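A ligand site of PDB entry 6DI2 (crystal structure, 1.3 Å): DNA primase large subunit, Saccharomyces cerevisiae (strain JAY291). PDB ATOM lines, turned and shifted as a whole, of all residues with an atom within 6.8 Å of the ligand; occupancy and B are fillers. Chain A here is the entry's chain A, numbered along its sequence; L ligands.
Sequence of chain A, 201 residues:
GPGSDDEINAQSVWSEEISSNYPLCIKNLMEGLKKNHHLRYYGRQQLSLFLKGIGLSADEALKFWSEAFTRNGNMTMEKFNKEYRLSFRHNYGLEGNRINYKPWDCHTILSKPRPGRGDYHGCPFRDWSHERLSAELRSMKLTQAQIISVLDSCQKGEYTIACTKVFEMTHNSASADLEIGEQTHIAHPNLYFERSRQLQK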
ATOM      1  N   PRO A  23      16.665   5.131 -35.446  1.00  0.00           N
ATOM      2  CA  PRO A  23      17.172   5.366 -34.084  1.00  0.00           C
ATOM      3  C   PRO A  23      18.636   5.770 -34.121  1.00  0.00           C
ATOM      4  O   PRO A  23      19.322   5.666 -35.154  1.00  0.00           O
ATOM      5  CB  PRO A  23      16.930   4.027 -33.409  1.00  0.00           C
ATOM      6  CG  PRO A  23      17.090   3.040 -34.518  1.00  0.00           C
ATOM      7  CD  PRO A  23      16.485   3.693 -35.752  1.00  0.00           C
ATOM      8  N   LEU A  24      19.174   6.147 -32.951  1.00  0.00           N
ATOM      9  CA  LEU A  24      20.516   6.728 -32.947  1.00  0.00           C
ATOM     10  C   LEU A  24      21.576   5.752 -33.441  1.00  0.00           C
ATOM     11  O   LEU A  24      22.538   6.175 -34.075  1.00  0.00           O
ATOM     12  CB  LEU A  24      20.943   7.252 -31.554  1.00  0.00           C
ATOM     13  CG  LEU A  24      20.296   8.500 -30.992  1.00  0.00           C
ATOM     14  CD1 LEU A  24      21.096   9.008 -29.794  1.00  0.00           C
ATOM     15  CD2 LEU A  24      20.202   9.542 -32.079  1.00  0.00           C
ATOM     16  N   CYS A  25      21.448   4.460 -33.123  1.00  0.00           N
ATOM     17  CA  CYS A  25      22.475   3.517 -33.584  1.00  0.00           C
ATOM     18  C   CYS A  25      22.555   3.490 -35.114  1.00  0.00           C
ATOM     19  O   CYS A  25      23.666   3.490 -35.679  1.00  0.00           O
ATOM     20  CB  CYS A  25      22.221   2.112 -33.024  1.00  0.00           C
ATOM     21  SG  CYS A  25      20.563   1.412 -33.376  1.00  0.00           S
ATOM     22  N   ILE A  26      21.400   3.459 -35.784  1.00  0.00           N
ATOM     23  CA  ILE A  26      21.379   3.426 -37.235  1.00  0.00           C
ATOM     24  C   ILE A  26      21.880   4.752 -37.789  1.00  0.00           C
ATOM     25  O   ILE A  26      22.595   4.768 -38.792  1.00  0.00           O
ATOM     26  CB  ILE A  26      19.993   3.019 -37.766  1.00  0.00           C
ATOM     27  CG1 ILE A  26      19.613   1.604 -37.234  1.00  0.00           C
ATOM     28  CG2 ILE A  26      19.895   3.120 -39.272  1.00  0.00           C
ATOM     29  CD1 ILE A  26      20.621   0.490 -37.497  1.00  0.00           C
ATOM     30  N   GLN A  46      25.232  -5.000 -38.438  1.00  0.00           N
ATOM     31  CA  GLN A  46      24.138  -4.295 -37.771  1.00  0.00           C
ATOM     32  C   GLN A  46      23.333  -3.488 -38.789  1.00  0.00           C
ATOM     33  O   GLN A  46      22.084  -3.547 -38.831  1.00  0.00           O
ATOM     34  CB  GLN A  46      24.703  -3.401 -36.682  1.00  0.00           C
ATOM     35  CG  GLN A  46      23.595  -2.768 -35.802  1.00  0.00           C
ATOM     36  CD  GLN A  46      24.178  -2.064 -34.590  1.00  0.00           C
ATOM     37  OE1 GLN A  46      25.294  -2.347 -34.143  1.00  0.00           O
ATOM     38  NE2 GLN A  46      23.388  -1.133 -34.011  1.00  0.00           N
ATOM     39  N   ASP A 105      18.045  -7.217 -32.581  1.00  0.00           N
ATOM     40  CA  ASP A 105      17.312  -6.430 -31.596  1.00  0.00           C
ATOM     41  C   ASP A 105      18.268  -5.699 -30.649  1.00  0.00           C
ATOM     42  O   ASP A 105      19.483  -5.866 -30.718  1.00  0.00           O
ATOM     43  CB  ASP A 105      16.242  -7.278 -30.902  1.00  0.00           C
ATOM     44  CG  ASP A 105      16.775  -8.313 -29.998  1.00  0.00           C
ATOM     45  OD1 ASP A 105      17.950  -8.385 -29.697  1.00  0.00           O
ATOM     46  OD2 ASP A 105      15.957  -9.121 -29.528  1.00  0.00           O
ATOM     47  N   CYS A 106      17.717  -4.837 -29.746  1.00  0.00           N
ATOM     48  CA  CYS A 106      18.610  -4.044 -28.916  1.00  0.00           C
ATOM     49  C   CYS A 106      19.438  -4.920 -27.982  1.00  0.00           C
ATOM     50  O   CYS A 106      20.632  -4.643 -27.760  1.00  0.00           O
ATOM     51  CB  CYS A 106      17.831  -3.049 -28.069  1.00  0.00           C
ATOM     52  SG  CYS A 106      16.889  -1.875 -29.133  1.00  0.00           S
ATOM     53  N   HIS A 107      18.838  -5.965 -27.397  1.00  0.00           N
ATOM     54  CA  HIS A 107      19.613  -6.824 -26.518  1.00  0.00           C
ATOM     55  C   HIS A 107      20.769  -7.454 -27.286  1.00  0.00           C
ATOM     56  O   HIS A 107      21.889  -7.550 -26.771  1.00  0.00           O
ATOM     57  CB  HIS A 107      18.685  -7.884 -25.934  1.00  0.00           C
ATOM     58  CG  HIS A 107      19.383  -8.843 -25.022  1.00  0.00           C
ATOM     59  ND1 HIS A 107      19.629  -8.580 -23.698  1.00  0.00           N
ATOM     60  CD2 HIS A 107      19.934 -10.053 -25.285  1.00  0.00           C
ATOM     61  CE1 HIS A 107      20.281  -9.611 -23.161  1.00  0.00           C
ATOM     62  NE2 HIS A 107      20.476 -10.504 -24.109  1.00  0.00           N
ATOM     63  N   ILE A 109      22.271  -6.231 -30.006  1.00  0.00           N
ATOM     64  CA  ILE A 109      23.247  -5.166 -30.259  1.00  0.00           C
ATOM     65  C   ILE A 109      24.099  -4.895 -29.033  1.00  0.00           C
ATOM     66  O   ILE A 109      25.331  -4.809 -29.114  1.00  0.00           O
ATOM     67  CB  ILE A 109      22.529  -3.905 -30.729  1.00  0.00           C
ATOM     68  CG1 ILE A 109      22.026  -4.134 -32.163  1.00  0.00           C
ATOM     69  CG2 ILE A 109      23.442  -2.694 -30.657  1.00  0.00           C
ATOM     70  CD1 ILE A 109      20.915  -3.151 -32.565  1.00  0.00           C
ATOM     71  N   LEU A 110      23.446  -4.747 -27.856  1.00  0.00           N
ATOM     72  CA  LEU A 110      24.165  -4.414 -26.642  1.00  0.00           C
ATOM     73  C   LEU A 110      25.098  -5.545 -26.232  1.00  0.00           C
ATOM     74  O   LEU A 110      26.117  -5.285 -25.588  1.00  0.00           O
ATOM     75  CB  LEU A 110      23.130  -4.094 -25.513  1.00  0.00           C
ATOM     76  CG  LEU A 110      22.472  -2.728 -25.683  1.00  0.00           C
ATOM     77  CD1 LEU A 110      21.166  -2.637 -24.866  1.00  0.00           C
ATOM     78  CD2 LEU A 110      23.403  -1.604 -25.325  1.00  0.00           C
ATOM     79  N   GLY A 122      26.884  -0.872 -32.150  1.00  0.00           N
ATOM     80  CA  GLY A 122      26.572  -0.710 -30.748  1.00  0.00           C
ATOM     81  C   GLY A 122      25.363   0.192 -30.562  1.00  0.00           C
ATOM     82  O   GLY A 122      24.516   0.336 -31.442  1.00  0.00           O
ATOM     83  N   CYS A 123      25.275   0.766 -29.357  1.00  0.00           N
ATOM     84  CA  CYS A 123      24.150   1.599 -28.943  1.00  0.00           C
ATOM     85  C   CYS A 123      24.710   2.920 -28.424  1.00  0.00           C
ATOM     86  O   CYS A 123      25.383   2.937 -27.375  1.00  0.00           O
ATOM     87  CB  CYS A 123      23.360   0.915 -27.828  1.00  0.00           C
ATOM     88  SG  CYS A 123      22.026   2.002 -27.211  1.00  0.00           S
ATOM     89  N   PRO A 124      24.493   4.024 -29.137  1.00  0.00           N
ATOM     90  CA  PRO A 124      25.061   5.314 -28.692  1.00  0.00           C
ATOM     91  C   PRO A 124      24.668   5.709 -27.286  1.00  0.00           C
ATOM     92  O   PRO A 124      25.431   6.450 -26.646  1.00  0.00           O
ATOM     93  CB  PRO A 124      24.530   6.296 -29.739  1.00  0.00           C
ATOM     94  CG  PRO A 124      24.465   5.418 -31.019  1.00  0.00           C
ATOM     95  CD  PRO A 124      23.901   4.113 -30.489  1.00  0.00           C
ATOM     96  N   PHE A 125      23.495   5.312 -26.785  1.00  0.00           N
ATOM     97  CA  PHE A 125      23.125   5.723 -25.430  1.00  0.00           C
ATOM     98  C   PHE A 125      24.093   5.155 -24.404  1.00  0.00           C
ATOM     99  O   PHE A 125      24.254   5.737 -23.334  1.00  0.00           O
ATOM    100  CB  PHE A 125      21.693   5.297 -25.154  1.00  0.00           C
ATOM    101  CG  PHE A 125      20.714   6.045 -26.029  1.00  0.00           C
ATOM    102  CD1 PHE A 125      20.448   7.408 -25.757  1.00  0.00           C
ATOM    103  CD2 PHE A 125      20.108   5.443 -27.128  1.00  0.00           C
ATOM    104  CE1 PHE A 125      19.557   8.113 -26.522  1.00  0.00           C
ATOM    105  CE2 PHE A 125      19.234   6.129 -27.914  1.00  0.00           C
ATOM    106  CZ  PHE A 125      18.950   7.457 -27.626  1.00  0.00           C
ATOM    107  N   ARG A 126      24.729   4.024 -24.720  1.00  0.00           N
ATOM    108  CA  ARG A 126      25.782   3.460 -23.903  1.00  0.00           C
ATOM    109  C   ARG A 126      27.153   3.938 -24.312  1.00  0.00           C
ATOM    110  O   ARG A 126      28.020   4.177 -23.461  1.00  0.00           O
ATOM    111  CB  ARG A 126      25.736   1.935 -23.962  1.00  0.00           C
ATOM    112  CG  ARG A 126      26.855   1.289 -23.121  1.00  0.00           C
ATOM    113  CD  ARG A 126      26.900  -0.192 -23.387  1.00  0.00           C
ATOM    114  NE  ARG A 126      27.366  -0.387 -24.767  1.00  0.00           N
ATOM    115  CZ  ARG A 126      27.316  -1.522 -25.455  1.00  0.00           C
ATOM    116  NH1 ARG A 126      26.913  -2.656 -24.866  1.00  0.00           N
ATOM    117  NH2 ARG A 126      27.731  -1.546 -26.731  1.00  0.00           N
ATOM    118  N   TYR A 159      19.425   1.851 -21.369  1.00  0.00           N
ATOM    119  CA  TYR A 159      19.629   2.409 -22.700  1.00  0.00           C
ATOM    120  C   TYR A 159      18.366   2.385 -23.544  1.00  0.00           C
ATOM    121  O   TYR A 159      18.115   3.323 -24.296  1.00  0.00           O
ATOM    122  CB  TYR A 159      20.802   1.690 -23.403  1.00  0.00           C
ATOM    123  CG  TYR A 159      22.001   1.663 -22.518  1.00  0.00           C
ATOM    124  CD1 TYR A 159      22.569   2.848 -22.059  1.00  0.00           C
ATOM    125  CD2 TYR A 159      22.560   0.417 -22.095  1.00  0.00           C
ATOM    126  CE1 TYR A 159      23.623   2.837 -21.150  1.00  0.00           C
ATOM    127  CE2 TYR A 159      23.646   0.401 -21.236  1.00  0.00           C
ATOM    128  CZ  TYR A 159      24.174   1.634 -20.754  1.00  0.00           C
ATOM    129  OH  TYR A 159      25.244   1.608 -19.879  1.00  0.00           O
ATOM    130  N   THR A 160      17.590   1.307 -23.482  1.00  0.00           N
ATOM    131  CA  THR A 160      16.382   1.230 -24.286  1.00  0.00           C
ATOM    132  C   THR A 160      15.311   2.207 -23.783  1.00  0.00           C
ATOM    133  O   THR A 160      14.514   2.671 -24.592  1.00  0.00           O
ATOM    134  CB  THR A 160      15.844  -0.201 -24.401  1.00  0.00           C
ATOM    135  OG1 THR A 160      15.485  -0.668 -23.080  1.00  0.00           O
ATOM    136  CG2 THR A 160      16.883  -1.111 -24.996  1.00  0.00           C
ATOM    137  N   ILE A 161      15.298   2.525 -22.476  1.00  0.00           N
ATOM    138  CA  ILE A 161      14.404   3.570 -22.004  1.00  0.00           C
ATOM    139  C   ILE A 161      14.860   4.937 -22.483  1.00  0.00           C
ATOM    140  O   ILE A 161      14.037   5.765 -22.887  1.00  0.00           O
ATOM    141  CB  ILE A 161      14.305   3.538 -20.455  1.00  0.00           C
ATOM    142  CG1 ILE A 161      13.610   2.228 -20.002  1.00  0.00           C
ATOM    143  CG2 ILE A 161      13.533   4.794 -19.953  1.00  0.00           C
ATOM    144  CD1 ILE A 161      13.464   2.062 -18.513  1.00  0.00           C
ATOM    145  N   ALA A 162      16.195   5.179 -22.508  1.00  0.00           N
ATOM    146  CA  ALA A 162      16.694   6.428 -23.064  1.00  0.00           C
ATOM    147  C   ALA A 162      16.239   6.594 -24.505  1.00  0.00           C
ATOM    148  O   ALA A 162      15.770   7.668 -24.919  1.00  0.00           O
ATOM    149  CB  ALA A 162      18.210   6.470 -22.990  1.00  0.00           C
ATOM    150  N   CYS A 163      16.347   5.510 -25.277  1.00  0.00           N
ATOM    151  CA  CYS A 163      15.955   5.549 -26.682  1.00  0.00           C
ATOM    152  C   CYS A 163      14.455   5.754 -26.836  1.00  0.00           C
ATOM    153  O   CYS A 163      13.999   6.543 -27.702  1.00  0.00           O
ATOM    154  CB  CYS A 163      16.434   4.205 -27.265  1.00  0.00           C
ATOM    155  SG  CYS A 163      16.177   4.091 -29.095  1.00  0.00           S
ATOM    156  N   THR A 164      13.656   5.116 -25.958  1.00  0.00           N
ATOM    157  CA  THR A 164      12.203   5.330 -25.970  1.00  0.00           C
ATOM    158  C   THR A 164      11.859   6.786 -25.660  1.00  0.00           C
ATOM    159  O   THR A 164      10.958   7.372 -26.289  1.00  0.00           O
ATOM    160  CB  THR A 164      11.552   4.390 -24.953  1.00  0.00           C
ATOM    161  OG1 THR A 164      11.824   3.033 -25.296  1.00  0.00           O
ATOM    162  CG2 THR A 164      10.049   4.572 -24.943  1.00  0.00           C
ATOM    163  N   ALA A 187      12.451  -4.429 -27.324  1.00  0.00           N
ATOM    164  CA  ALA A 187      13.308  -3.342 -27.820  1.00  0.00           C
ATOM    165  C   ALA A 187      14.027  -3.782 -29.121  1.00  0.00           C
ATOM    166  O   ALA A 187      14.746  -4.702 -29.124  1.00  0.00           O
ATOM    167  CB  ALA A 187      14.300  -3.015 -26.776  1.00  0.00           C
ATOM    168  N   HIS A 188      13.770  -2.997 -30.125  1.00  0.00           N
ATOM    169  CA  HIS A 188      14.287  -3.341 -31.457  1.00  0.00           C
ATOM    170  C   HIS A 188      14.451  -2.107 -32.342  1.00  0.00           C
ATOM    171  O   HIS A 188      13.508  -1.408 -32.530  1.00  0.00           O
ATOM    172  CB  HIS A 188      13.311  -4.308 -32.110  1.00  0.00           C
ATOM    173  CG  HIS A 188      13.923  -5.154 -33.164  1.00  0.00           C
ATOM    174  ND1 HIS A 188      14.529  -4.629 -34.266  1.00  0.00           N
ATOM    175  CD2 HIS A 188      13.948  -6.486 -33.285  1.00  0.00           C
ATOM    176  CE1 HIS A 188      14.916  -5.597 -34.986  1.00  0.00           C
ATOM    177  NE2 HIS A 188      14.571  -6.745 -34.438  1.00  0.00           N
ATOM    178  N   PRO A 189      15.637  -1.893 -32.958  1.00  0.00           N
ATOM    179  CA  PRO A 189      15.770  -0.745 -33.857  1.00  0.00           C
ATOM    180  C   PRO A 189      14.744  -0.753 -34.972  1.00  0.00           C
ATOM    181  O   PRO A 189      14.293   0.325 -35.431  1.00  0.00           O
ATOM    182  CB  PRO A 189      17.199  -0.868 -34.414  1.00  0.00           C
ATOM    183  CG  PRO A 189      17.930  -1.736 -33.421  1.00  0.00           C
ATOM    184  CD  PRO A 189      16.884  -2.660 -32.841  1.00  0.00           C
ATOM    185  N   ASN A 190      14.357  -1.937 -35.470  1.00  0.00           N
ATOM    186  CA  ASN A 190      13.367  -1.975 -36.538  1.00  0.00           C
ATOM    187  C   ASN A 190      11.986  -1.549 -36.053  1.00  0.00           C
ATOM    188  O   ASN A 190      11.189  -1.054 -36.833  1.00  0.00           O
ATOM    189  CB  ASN A 190      13.344  -3.341 -37.229  1.00  0.00           C
ATOM    190  CG  ASN A 190      14.559  -3.536 -38.108  1.00  0.00           C
ATOM    191  OD1 ASN A 190      15.628  -3.885 -37.597  1.00  0.00           O
ATOM    192  ND2 ASN A 190      14.434  -3.261 -39.404  1.00  0.00           N
ATOM    193  N   TYR A 192      11.580   0.804 -33.681  1.00  0.00           N
ATOM    194  CA  TYR A 192      11.695   2.254 -33.685  1.00  0.00           C
ATOM    195  C   TYR A 192      11.386   2.793 -35.058  1.00  0.00           C
ATOM    196  O   TYR A 192      10.560   3.714 -35.236  1.00  0.00           O
ATOM    197  CB  TYR A 192      13.096   2.637 -33.242  1.00  0.00           C
ATOM    198  CG  TYR A 192      13.339   4.082 -32.908  1.00  0.00           C
ATOM    199  CD1 TYR A 192      13.329   5.089 -33.891  1.00  0.00           C
ATOM    200  CD2 TYR A 192      13.642   4.446 -31.584  1.00  0.00           C
ATOM    201  CE1 TYR A 192      13.616   6.393 -33.571  1.00  0.00           C
ATOM    202  CE2 TYR A 192      13.908   5.751 -31.247  1.00  0.00           C
ATOM    203  CZ  TYR A 192      13.912   6.725 -32.232  1.00  0.00           C
ATOM    204  OH  TYR A 192      14.239   7.992 -31.838  1.00  0.00           O
HETATM  205 FE1  LIG L   1      19.607   1.357 -31.310  1.00  0.00          FE
HETATM  206 FE2  LIG L   1      18.274  -0.076 -29.385  1.00  0.00          FE
HETATM  207 FE3  LIG L   1      17.881   2.606 -29.573  1.00  0.00          FE
HETATM  208 FE4  LIG L   1      20.272   1.638 -28.667  1.00  0.00          FE
HETATM  209  S1  LIG L   1      18.299   1.401 -27.638  1.00  0.00           S
HETATM  210  S2  LIG L   1      19.944   3.373 -30.213  1.00  0.00           S
HETATM  211  S3  LIG L   1      20.473  -0.289 -29.908  1.00  0.00           S
HETATM  212  S4  LIG L   1      17.381   1.094 -31.194  1.00  0.00           S
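The backbone NH (N) of Cys 25 lies close to a sulfur (S2) of the ligand, 3.5 Å away.
FE3 of the ligand is bound by SG of Cys 163 (2.3 Å).
The side-chain sulfur (SG) of Cys 123 is bound to an iron atom (FE4) of the ligand, at 2.3 Å.
An iron atom (FE2) of the ligand is bound by the side-chain sulfur (SG) of Cys 106, 2.3 Å away.
An iron atom (FE1) of the ligand is bound by the side-chain sulfur (SG) of Cys 25.
N of His 188 sits close to SG of Cys 106 (3.5 Å).
The side-chain sulfur (SG) of Cys 123 sits close to the backbone NH (N) of Phe 125 (3.6 Å).
The backbone NH (N) of Cys 106 is in hydrogen-bond range of the backbone carbonyl oxygen (O) of Ala 187.
OG1 of Thr 164 lies within hydrogen-bond range of O of Thr 160, at 2.8 Å.
Residues that only touch the ligand: Pro 189 (3.6 Å), Phe 125 (3.7 Å), Pro 23 (3.7 Å), Tyr 159 (3.9 Å), Thr 160 (3.9 Å), Ile 109 (3.9 Å) and Leu 24 (3.97 Å).
Within 4 Å of the ligand: Pro 23, Leu 24, Cys 25, Cys 106, Ile 109, Cys 123, Phe 125, Tyr 159, Thr 160, Cys 163 and Pro 189.
The nearest printed residue that does not touch the ligand is Pro 124 (4.04 Å).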
